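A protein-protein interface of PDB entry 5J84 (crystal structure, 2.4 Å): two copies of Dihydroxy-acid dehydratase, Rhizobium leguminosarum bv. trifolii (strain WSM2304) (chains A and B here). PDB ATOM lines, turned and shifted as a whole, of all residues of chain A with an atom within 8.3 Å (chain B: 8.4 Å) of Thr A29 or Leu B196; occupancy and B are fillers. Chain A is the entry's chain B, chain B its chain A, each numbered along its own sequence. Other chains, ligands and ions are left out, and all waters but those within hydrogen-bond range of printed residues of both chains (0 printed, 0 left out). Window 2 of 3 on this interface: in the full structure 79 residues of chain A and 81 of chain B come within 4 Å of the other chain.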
ATOM      1  N   GLN A  23      -2.730 -16.557 -22.441  1.00  0.00           N
ATOM      2  CA  GLN A  23      -1.601 -17.477 -22.588  1.00  0.00           C
ATOM      3  C   GLN A  23      -1.751 -18.751 -21.750  1.00  0.00           C
ATOM      4  O   GLN A  23      -1.041 -19.731 -21.975  1.00  0.00           O
ATOM      5  CB  GLN A  23      -0.295 -16.771 -22.211  1.00  0.00           C
ATOM      6  CG  GLN A  23       0.199 -15.765 -23.238  1.00  0.00           C
ATOM      7  CD  GLN A  23       0.746 -16.419 -24.489  1.00  0.00           C
ATOM      8  OE1 GLN A  23       1.925 -16.770 -24.556  1.00  0.00           O
ATOM      9  NE2 GLN A  23      -0.109 -16.588 -25.491  1.00  0.00           N
ATOM     10  N   TRP A  25      -4.289 -20.462 -22.024  1.00  0.00           N
ATOM     11  CA  TRP A  25      -4.896 -21.307 -23.035  1.00  0.00           C
ATOM     12  C   TRP A  25      -3.920 -21.557 -24.175  1.00  0.00           C
ATOM     13  O   TRP A  25      -3.787 -22.679 -24.660  1.00  0.00           O
ATOM     14  CB  TRP A  25      -6.163 -20.664 -23.600  1.00  0.00           C
ATOM     15  CG  TRP A  25      -7.384 -20.701 -22.729  1.00  0.00           C
ATOM     16  CD1 TRP A  25      -8.396 -21.612 -22.785  1.00  0.00           C
ATOM     17  CD2 TRP A  25      -7.756 -19.748 -21.723  1.00  0.00           C
ATOM     18  NE1 TRP A  25      -9.362 -21.304 -21.858  1.00  0.00           N
ATOM     19  CE2 TRP A  25      -8.994 -20.162 -21.195  1.00  0.00           C
ATOM     20  CE3 TRP A  25      -7.156 -18.595 -21.207  1.00  0.00           C
ATOM     21  CZ2 TRP A  25      -9.643 -19.464 -20.175  1.00  0.00           C
ATOM     22  CZ3 TRP A  25      -7.803 -17.902 -20.198  1.00  0.00           C
ATOM     23  CH2 TRP A  25      -9.035 -18.338 -19.693  1.00  0.00           C
ATOM     24  N   TYR A  26      -3.235 -20.496 -24.596  1.00  0.00           N
ATOM     25  CA  TYR A  26      -2.543 -20.499 -25.882  1.00  0.00           C
ATOM     26  C   TYR A  26      -1.026 -20.352 -25.803  1.00  0.00           C
ATOM     27  O   TYR A  26      -0.345 -20.396 -26.826  1.00  0.00           O
ATOM     28  CB  TYR A  26      -3.109 -19.383 -26.762  1.00  0.00           C
ATOM     29  CG  TYR A  26      -4.586 -19.526 -27.040  1.00  0.00           C
ATOM     30  CD1 TYR A  26      -5.131 -20.761 -27.360  1.00  0.00           C
ATOM     31  CD2 TYR A  26      -5.432 -18.428 -26.993  1.00  0.00           C
ATOM     32  CE1 TYR A  26      -6.476 -20.900 -27.620  1.00  0.00           C
ATOM     33  CE2 TYR A  26      -6.782 -18.558 -27.252  1.00  0.00           C
ATOM     34  CZ  TYR A  26      -7.299 -19.799 -27.566  1.00  0.00           C
ATOM     35  OH  TYR A  26      -8.641 -19.942 -27.826  1.00  0.00           O
ATOM     36  N   GLY A  27      -0.496 -20.178 -24.600  1.00  0.00           N
ATOM     37  CA  GLY A  27       0.941 -20.060 -24.433  1.00  0.00           C
ATOM     38  C   GLY A  27       1.578 -21.324 -23.889  1.00  0.00           C
ATOM     39  O   GLY A  27       1.149 -21.853 -22.866  1.00  0.00           O
ATOM     40  N   GLY A  28       2.602 -21.817 -24.574  1.00  0.00           N
ATOM     41  CA  GLY A  28       3.336 -22.970 -24.086  1.00  0.00           C
ATOM     42  C   GLY A  28       3.394 -24.132 -25.057  1.00  0.00           C
ATOM     43  O   GLY A  28       3.136 -23.976 -26.247  1.00  0.00           O
ATOM     44  N   THR A  29       3.731 -25.307 -24.539  1.00  0.00           N
ATOM     45  CA  THR A  29       3.953 -26.483 -25.375  1.00  0.00           C
ATOM     46  C   THR A  29       3.216 -27.719 -24.858  1.00  0.00           C
ATOM     47  O   THR A  29       3.337 -28.802 -25.428  1.00  0.00           O
ATOM     48  CB  THR A  29       5.453 -26.808 -25.486  1.00  0.00           C
ATOM     49  OG1 THR A  29       5.993 -27.005 -24.173  1.00  0.00           O
ATOM     50  CG2 THR A  29       6.201 -25.667 -26.151  1.00  0.00           C
ATOM     51  N   SER A  30       2.467 -27.554 -23.772  1.00  0.00           N
ATOM     52  CA  SER A  30       1.752 -28.663 -23.147  1.00  0.00           C
ATOM     53  C   SER A  30       0.649 -29.215 -24.046  1.00  0.00           C
ATOM     54  O   SER A  30       0.281 -28.599 -25.046  1.00  0.00           O
ATOM     55  CB  SER A  30       1.147 -28.228 -21.812  1.00  0.00           C
ATOM     56  OG  SER A  30       0.093 -27.300 -22.007  1.00  0.00           O
ATOM     57  N   ARG A  31       0.137 -30.386 -23.680  1.00  0.00           N
ATOM     58  CA  ARG A  31      -0.967 -31.011 -24.397  1.00  0.00           C
ATOM     59  C   ARG A  31      -2.182 -30.090 -24.461  1.00  0.00           C
ATOM     60  O   ARG A  31      -2.866 -30.026 -25.483  1.00  0.00           O
ATOM     61  CB  ARG A  31      -1.359 -32.331 -23.731  1.00  0.00           C
ATOM     62  CG  ARG A  31      -2.532 -33.038 -24.395  1.00  0.00           C
ATOM     63  CD  ARG A  31      -3.083 -34.118 -23.489  1.00  0.00           C
ATOM     64  NE  ARG A  31      -3.655 -33.532 -22.281  1.00  0.00           N
ATOM     65  CZ  ARG A  31      -3.983 -34.221 -21.195  1.00  0.00           C
ATOM     66  NH1 ARG A  31      -3.795 -35.532 -21.156  1.00  0.00           N
ATOM     67  NH2 ARG A  31      -4.494 -33.593 -20.145  1.00  0.00           N
ATOM     68  N   ASP A  32      -2.448 -29.390 -23.361  1.00  0.00           N
ATOM     69  CA  ASP A  32      -3.610 -28.510 -23.266  1.00  0.00           C
ATOM     70  C   ASP A  32      -3.506 -27.342 -24.235  1.00  0.00           C
ATOM     71  O   ASP A  32      -4.497 -26.938 -24.841  1.00  0.00           O
ATOM     72  CB  ASP A  32      -3.779 -27.986 -21.839  1.00  0.00           C
ATOM     73  CG  ASP A  32      -4.137 -29.080 -20.856  1.00  0.00           C
ATOM     74  OD1 ASP A  32      -4.893 -29.995 -21.240  1.00  0.00           O
ATOM     75  OD2 ASP A  32      -3.660 -29.027 -19.703  1.00  0.00           O
ATOM     76  N   VAL A  33      -2.300 -26.812 -24.386  1.00  0.00           N
ATOM     77  CA  VAL A  33      -2.076 -25.691 -25.288  1.00  0.00           C
ATOM     78  C   VAL A  33      -2.213 -26.158 -26.731  1.00  0.00           C
ATOM     79  O   VAL A  33      -2.764 -25.451 -27.571  1.00  0.00           O
ATOM     80  CB  VAL A  33      -0.691 -25.061 -25.068  1.00  0.00           C
ATOM     81  CG1 VAL A  33      -0.448 -23.956 -26.071  1.00  0.00           C
ATOM     82  CG2 VAL A  33      -0.577 -24.528 -23.647  1.00  0.00           C
ATOM     83  N   ILE A  34      -1.718 -27.361 -27.004  1.00  0.00           N
ATOM     84  CA  ILE A  34      -1.876 -27.980 -28.312  1.00  0.00           C
ATOM     85  C   ILE A  34      -3.362 -28.173 -28.619  1.00  0.00           C
ATOM     86  O   ILE A  34      -3.800 -28.005 -29.756  1.00  0.00           O
ATOM     87  CB  ILE A  34      -1.140 -29.337 -28.382  1.00  0.00           C
ATOM     88  CG1 ILE A  34       0.369 -29.133 -28.230  1.00  0.00           C
ATOM     89  CG2 ILE A  34      -1.450 -30.061 -29.687  1.00  0.00           C
ATOM     90  CD1 ILE A  34       1.159 -30.422 -28.166  1.00  0.00           C
ATOM     91  N   TYR A  35      -4.134 -28.512 -27.591  1.00  0.00           N
ATOM     92  CA  TYR A  35      -5.578 -28.675 -27.721  1.00  0.00           C
ATOM     93  C   TYR A  35      -6.262 -27.336 -28.008  1.00  0.00           C
ATOM     94  O   TYR A  35      -6.984 -27.197 -28.992  1.00  0.00           O
ATOM     95  CB  TYR A  35      -6.151 -29.313 -26.446  1.00  0.00           C
ATOM     96  CG  TYR A  35      -7.667 -29.359 -26.364  1.00  0.00           C
ATOM     97  CD1 TYR A  35      -8.409 -30.153 -27.230  1.00  0.00           C
ATOM     98  CD2 TYR A  35      -8.354 -28.622 -25.405  1.00  0.00           C
ATOM     99  CE1 TYR A  35      -9.791 -30.203 -27.150  1.00  0.00           C
ATOM    100  CE2 TYR A  35      -9.736 -28.665 -25.319  1.00  0.00           C
ATOM    101  CZ  TYR A  35     -10.451 -29.457 -26.195  1.00  0.00           C
ATOM    102  OH  TYR A  35     -11.827 -29.505 -26.114  1.00  0.00           O
ATOM    103  N   ARG A  37      -4.913 -24.190 -28.770  1.00  0.00           N
ATOM    104  CA  ARG A  37      -4.385 -23.482 -29.933  1.00  0.00           C
ATOM    105  C   ARG A  37      -4.676 -24.239 -31.227  1.00  0.00           C
ATOM    106  O   ARG A  37      -5.040 -23.641 -32.240  1.00  0.00           O
ATOM    107  CB  ARG A  37      -2.879 -23.261 -29.796  1.00  0.00           C
ATOM    108  CG  ARG A  37      -2.334 -22.258 -30.777  1.00  0.00           C
ATOM    109  CD  ARG A  37      -0.854 -22.454 -31.045  1.00  0.00           C
ATOM    110  NE  ARG A  37      -0.026 -22.374 -29.848  1.00  0.00           N
ATOM    111  CZ  ARG A  37       0.835 -23.315 -29.479  1.00  0.00           C
ATOM    112  NH1 ARG A  37       0.980 -24.407 -30.215  1.00  0.00           N
ATOM    113  NH2 ARG A  37       1.561 -23.163 -28.382  1.00  0.00           N
ATOM    114  N   LYS A  41      -7.060 -23.072 -34.585  1.00  0.00           N
ATOM    115  CA  LYS A  41      -6.379 -22.973 -35.871  1.00  0.00           C
ATOM    116  C   LYS A  41      -7.199 -23.538 -37.031  1.00  0.00           C
ATOM    117  O   LYS A  41      -6.862 -23.310 -38.191  1.00  0.00           O
ATOM    118  CB  LYS A  41      -5.026 -23.682 -35.804  1.00  0.00           C
ATOM    119  CG  LYS A  41      -3.922 -22.851 -35.168  1.00  0.00           C
ATOM    120  CD  LYS A  41      -2.620 -23.629 -35.110  1.00  0.00           C
ATOM    121  CE  LYS A  41      -1.493 -22.787 -34.539  1.00  0.00           C
ATOM    122  NZ  LYS A  41      -0.236 -23.578 -34.410  1.00  0.00           N
ATOM    123  N   HIS A  47       0.238 -18.802 -36.804  1.00  0.00           N
ATOM    124  CA  HIS A  47       0.687 -19.197 -35.470  1.00  0.00           C
ATOM    125  C   HIS A  47       1.048 -18.015 -34.565  1.00  0.00           C
ATOM    126  O   HIS A  47       0.830 -18.069 -33.354  1.00  0.00           O
ATOM    127  CB  HIS A  47       1.887 -20.141 -35.569  1.00  0.00           C
ATOM    128  CG  HIS A  47       2.410 -20.589 -34.239  1.00  0.00           C
ATOM    129  ND1 HIS A  47       1.664 -21.349 -33.366  1.00  0.00           N
ATOM    130  CD2 HIS A  47       3.600 -20.375 -33.631  1.00  0.00           C
ATOM    131  CE1 HIS A  47       2.375 -21.587 -32.277  1.00  0.00           C
ATOM    132  NE2 HIS A  47       3.553 -21.007 -32.413  1.00  0.00           N
ATOM    133  N   PHE B 167      -0.736 -36.992 -39.642  1.00  0.00           N
ATOM    134  CA  PHE B 167       0.616 -36.684 -39.181  1.00  0.00           C
ATOM    135  C   PHE B 167       1.607 -37.740 -39.650  1.00  0.00           C
ATOM    136  O   PHE B 167       1.516 -38.907 -39.259  1.00  0.00           O
ATOM    137  CB  PHE B 167       0.673 -36.564 -37.661  1.00  0.00           C
ATOM    138  CG  PHE B 167       2.027 -36.175 -37.137  1.00  0.00           C
ATOM    139  CD1 PHE B 167       2.642 -35.012 -37.574  1.00  0.00           C
ATOM    140  CD2 PHE B 167       2.684 -36.968 -36.211  1.00  0.00           C
ATOM    141  CE1 PHE B 167       3.886 -34.645 -37.095  1.00  0.00           C
ATOM    142  CE2 PHE B 167       3.929 -36.607 -35.728  1.00  0.00           C
ATOM    143  CZ  PHE B 167       4.531 -35.445 -36.171  1.00  0.00           C
ATOM    144  N   PHE B 181      -0.491 -39.378 -27.874  1.00  0.00           N
ATOM    145  CA  PHE B 181       0.806 -38.726 -28.020  1.00  0.00           C
ATOM    146  C   PHE B 181       1.382 -38.265 -26.682  1.00  0.00           C
ATOM    147  O   PHE B 181       2.571 -38.440 -26.423  1.00  0.00           O
ATOM    148  CB  PHE B 181       0.701 -37.537 -28.976  1.00  0.00           C
ATOM    149  CG  PHE B 181       0.562 -37.929 -30.417  1.00  0.00           C
ATOM    150  CD1 PHE B 181       0.925 -39.198 -30.840  1.00  0.00           C
ATOM    151  CD2 PHE B 181       0.080 -37.030 -31.351  1.00  0.00           C
ATOM    152  CE1 PHE B 181       0.805 -39.564 -32.168  1.00  0.00           C
ATOM    153  CE2 PHE B 181      -0.041 -37.388 -32.683  1.00  0.00           C
ATOM    154  CZ  PHE B 181       0.321 -38.657 -33.090  1.00  0.00           C
ATOM    155  N   VAL B 185       4.796 -39.496 -24.984  1.00  0.00           N
ATOM    156  CA  VAL B 185       5.840 -38.577 -24.548  1.00  0.00           C
ATOM    157  C   VAL B 185       6.315 -38.919 -23.136  1.00  0.00           C
ATOM    158  O   VAL B 185       7.512 -38.896 -22.854  1.00  0.00           O
ATOM    159  CB  VAL B 185       5.350 -37.107 -24.597  1.00  0.00           C
ATOM    160  CG1 VAL B 185       6.309 -36.183 -23.858  1.00  0.00           C
ATOM    161  CG2 VAL B 185       5.180 -36.652 -26.038  1.00  0.00           C
ATOM    162  N   MET B 190       8.273 -40.603 -27.444  1.00  0.00           N
ATOM    163  CA  MET B 190       7.998 -39.454 -28.301  1.00  0.00           C
ATOM    164  C   MET B 190       8.458 -38.179 -27.607  1.00  0.00           C
ATOM    165  O   MET B 190       8.402 -38.080 -26.382  1.00  0.00           O
ATOM    166  CB  MET B 190       6.506 -39.379 -28.639  1.00  0.00           C
ATOM    167  CG  MET B 190       6.131 -38.338 -29.688  1.00  0.00           C
ATOM    168  SD  MET B 190       4.343 -38.231 -29.924  1.00  0.00           S
ATOM    169  CE  MET B 190       4.242 -37.291 -31.445  1.00  0.00           C
ATOM    170  N   THR B 191       8.907 -37.203 -28.386  1.00  0.00           N
ATOM    171  CA  THR B 191       9.335 -35.933 -27.816  1.00  0.00           C
ATOM    172  C   THR B 191       8.196 -34.933 -27.885  1.00  0.00           C
ATOM    173  O   THR B 191       7.298 -35.063 -28.716  1.00  0.00           O
ATOM    174  CB  THR B 191      10.562 -35.357 -28.547  1.00  0.00           C
ATOM    175  OG1 THR B 191      10.176 -34.892 -29.847  1.00  0.00           O
ATOM    176  CG2 THR B 191      11.647 -36.416 -28.688  1.00  0.00           C
ATOM    177  N   GLN B 192       8.232 -33.936 -27.008  1.00  0.00           N
ATOM    178  CA  GLN B 192       7.224 -32.887 -27.029  1.00  0.00           C
ATOM    179  C   GLN B 192       7.353 -32.084 -28.315  1.00  0.00           C
ATOM    180  O   GLN B 192       6.376 -31.525 -28.808  1.00  0.00           O
ATOM    181  CB  GLN B 192       7.352 -31.976 -25.810  1.00  0.00           C
ATOM    182  CG  GLN B 192       6.151 -31.063 -25.608  1.00  0.00           C
ATOM    183  CD  GLN B 192       4.879 -31.829 -25.276  1.00  0.00           C
ATOM    184  OE1 GLN B 192       4.927 -32.952 -24.775  1.00  0.00           O
ATOM    185  NE2 GLN B 192       3.732 -31.222 -25.561  1.00  0.00           N
ATOM    186  N   ALA B 193       8.568 -32.037 -28.851  1.00  0.00           N
ATOM    187  CA  ALA B 193       8.821 -31.366 -30.120  1.00  0.00           C
ATOM    188  C   ALA B 193       8.044 -32.013 -31.263  1.00  0.00           C
ATOM    189  O   ALA B 193       7.456 -31.315 -32.088  1.00  0.00           O
ATOM    190  CB  ALA B 193      10.307 -31.368 -30.429  1.00  0.00           C
ATOM    191  N   GLU B 194       8.038 -33.342 -31.309  1.00  0.00           N
ATOM    192  CA  GLU B 194       7.291 -34.060 -32.342  1.00  0.00           C
ATOM    193  C   GLU B 194       5.792 -33.853 -32.176  1.00  0.00           C
ATOM    194  O   GLU B 194       5.052 -33.769 -33.154  1.00  0.00           O
ATOM    195  CB  GLU B 194       7.607 -35.556 -32.308  1.00  0.00           C
ATOM    196  CG  GLU B 194       9.006 -35.924 -32.758  1.00  0.00           C
ATOM    197  CD  GLU B 194       9.307 -37.392 -32.533  1.00  0.00           C
ATOM    198  OE1 GLU B 194       9.134 -37.865 -31.391  1.00  0.00           O
ATOM    199  OE2 GLU B 194       9.711 -38.074 -33.497  1.00  0.00           O
ATOM    200  N   PHE B 195       5.360 -33.771 -30.924  1.00  0.00           N
ATOM    201  CA  PHE B 195       3.962 -33.552 -30.596  1.00  0.00           C
ATOM    202  C   PHE B 195       3.536 -32.182 -31.134  1.00  0.00           C
ATOM    203  O   PHE B 195       2.451 -32.042 -31.697  1.00  0.00           O
ATOM    204  CB  PHE B 195       3.751 -33.669 -29.081  1.00  0.00           C
ATOM    205  CG  PHE B 195       2.310 -33.844 -28.664  1.00  0.00           C
ATOM    206  CD1 PHE B 195       1.290 -33.886 -29.601  1.00  0.00           C
ATOM    207  CD2 PHE B 195       1.983 -33.986 -27.324  1.00  0.00           C
ATOM    208  CE1 PHE B 195      -0.027 -34.048 -29.209  1.00  0.00           C
ATOM    209  CE2 PHE B 195       0.670 -34.152 -26.927  1.00  0.00           C
ATOM    210  CZ  PHE B 195      -0.337 -34.181 -27.871  1.00  0.00           C
ATOM    211  N   LEU B 196       4.399 -31.183 -30.970  1.00  0.00           N
ATOM    212  CA  LEU B 196       4.110 -29.832 -31.453  1.00  0.00           C
ATOM    213  C   LEU B 196       3.985 -29.795 -32.972  1.00  0.00           C
ATOM    214  O   LEU B 196       3.187 -29.035 -33.517  1.00  0.00           O
ATOM    215  CB  LEU B 196       5.192 -28.846 -31.005  1.00  0.00           C
ATOM    216  CG  LEU B 196       5.242 -28.460 -29.526  1.00  0.00           C
ATOM    217  CD1 LEU B 196       6.574 -27.804 -29.193  1.00  0.00           C
ATOM    218  CD2 LEU B 196       4.084 -27.535 -29.177  1.00  0.00           C
ATOM    219  N   GLU B 197       4.775 -30.625 -33.646  1.00  0.00           N
ATOM    220  CA  GLU B 197       4.761 -30.695 -35.103  1.00  0.00           C
ATOM    221  C   GLU B 197       3.436 -31.241 -35.633  1.00  0.00           C
ATOM    222  O   GLU B 197       3.029 -30.934 -36.751  1.00  0.00           O
ATOM    223  CB  GLU B 197       5.908 -31.578 -35.602  1.00  0.00           C
ATOM    224  CG  GLU B 197       7.301 -31.053 -35.307  1.00  0.00           C
ATOM    225  CD  GLU B 197       8.379 -32.094 -35.576  1.00  0.00           C
ATOM    226  OE1 GLU B 197       8.090 -33.091 -36.272  1.00  0.00           O
ATOM    227  OE2 GLU B 197       9.512 -31.917 -35.084  1.00  0.00           O
ATOM    228  N   ALA B 198       2.773 -32.058 -34.821  1.00  0.00           N
ATOM    229  CA  ALA B 198       1.513 -32.687 -35.206  1.00  0.00           C
ATOM    230  C   ALA B 198       0.325 -31.736 -35.117  1.00  0.00           C
ATOM    231  O   ALA B 198      -0.715 -31.969 -35.734  1.00  0.00           O
ATOM    232  CB  ALA B 198       1.261 -33.917 -34.345  1.00  0.00           C
ATOM    233  N   GLU B 199       0.485 -30.676 -34.334  1.00  0.00           N
ATOM    234  CA  GLU B 199      -0.594 -29.732 -34.055  1.00  0.00           C
ATOM    235  C   GLU B 199      -1.213 -29.095 -35.303  1.00  0.00           C
ATOM    236  O   GLU B 199      -2.428 -28.911 -35.380  1.00  0.00           O
ATOM    237  CB  GLU B 199      -0.085 -28.636 -33.120  1.00  0.00           C
ATOM    238  CG  GLU B 199      -1.135 -27.606 -32.758  1.00  0.00           C
ATOM    239  CD  GLU B 199      -0.573 -26.459 -31.955  1.00  0.00           C
ATOM    240  OE1 GLU B 199       0.259 -26.706 -31.056  1.00  0.00           O
ATOM    241  OE2 GLU B 199      -0.968 -25.311 -32.219  1.00  0.00           O
ATOM    242  N   ALA B 200      -0.372 -28.754 -36.272  1.00  0.00           N
ATOM    243  CA  ALA B 200      -0.812 -28.012 -37.449  1.00  0.00           C
ATOM    244  C   ALA B 200      -1.818 -28.767 -38.320  1.00  0.00           C
ATOM    245  O   ALA B 200      -2.763 -28.172 -38.837  1.00  0.00           O
ATOM    246  CB  ALA B 200       0.397 -27.616 -38.286  1.00  0.00           C
ATOM    247  N   SER B 201      -1.618 -30.070 -38.484  1.00  0.00           N
ATOM    248  CA  SER B 201      -2.447 -30.857 -39.392  1.00  0.00           C
ATOM    249  C   SER B 201      -3.438 -31.765 -38.666  1.00  0.00           C
ATOM    250  O   SER B 201      -3.925 -32.743 -39.231  1.00  0.00           O
ATOM    251  CB  SER B 201      -1.561 -31.694 -40.319  1.00  0.00           C
ATOM    252  OG  SER B 201      -0.609 -32.433 -39.578  1.00  0.00           O
ATOM    253  N   MET B 202      -3.736 -31.434 -37.414  1.00  0.00           N
ATOM    254  CA  MET B 202      -4.655 -32.230 -36.606  1.00  0.00           C
ATOM    255  C   MET B 202      -6.100 -31.739 -36.753  1.00  0.00           C
ATOM    256  O   MET B 202      -7.029 -32.537 -36.883  1.00  0.00           O
ATOM    257  CB  MET B 202      -4.221 -32.201 -35.139  1.00  0.00           C
ATOM    258  CG  MET B 202      -4.970 -33.166 -34.236  1.00  0.00           C
ATOM    259  SD  MET B 202      -4.242 -33.268 -32.586  1.00  0.00           S
ATOM    260  CE  MET B 202      -5.439 -34.309 -31.751  1.00  0.00           C
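Of the 15 printed residues of chain A, 5 touch a printed residue of chain B.
Hydrophobic or aromatic side chains of chain B within 4 Å of the printed part of chain A: Phe B195 and Leu B196.
The backbone carbonyl oxygen of Thr A29 sits at hydrogen-bond distance from the side-chain amide nitrogen of Gln B192, 2.5 Å away.
The guanidinium group (NH1) of Arg A37 lies within salt-bridge range of the side-chain carboxylate (OE1) of Glu B199.
OE2 of Glu B199 is in salt-bridge range of NZ of Lys A41 (2.9 Å).
Among the printed residues, merely in contact across the chains: Ile A34 with Phe B195 (3.6 Å), Ile A34 with Glu B199 (3.7 Å), Thr A29 with Leu B196 (3.7 Å), Ile A34 with Gln B192 (3.7 Å) and Ser A30 with Gln B192 (3.98 Å).
Of chain B, only Gln B192 and Leu B196 come within 4 Å of Thr A29.
Of chain A, only Thr A29 comes within 4 Å of Leu B196.
No residue of chain B comes within 4 Å of Gly A28.
Ser A30 touches just one residue of chain B: Gln B192.
Printed residues of chain A within 4 Å of Phe B195: Ile A34.
Of the printed residues of chain B, Arg A37 touches Glu B199 (2.6 Å).
Of the printed residues of chain A, Gln B192 touches Thr A29 (2.5 Å), Ser A30 (3.98 Å) and Ile A34 (3.7 Å).
Printed residues of chain B within 4 Å of Ile A34: Gln B192, Phe B195 and Glu B199.
The nearest residue of chain A that does not touch Leu B196 is Ile A34 (4.2 Å).
The backbone carbonyl oxygen (O) of Gly A28 is in hydrogen-bond range of the guanidinium group (NH2) of Arg A37.
OG of Ser A30 sits close to N of Val A33.
ND1 of His A47 sits at hydrogen-bond distance from NZ of Lys A41 (3.1 Å).
No position is printed for both chains.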
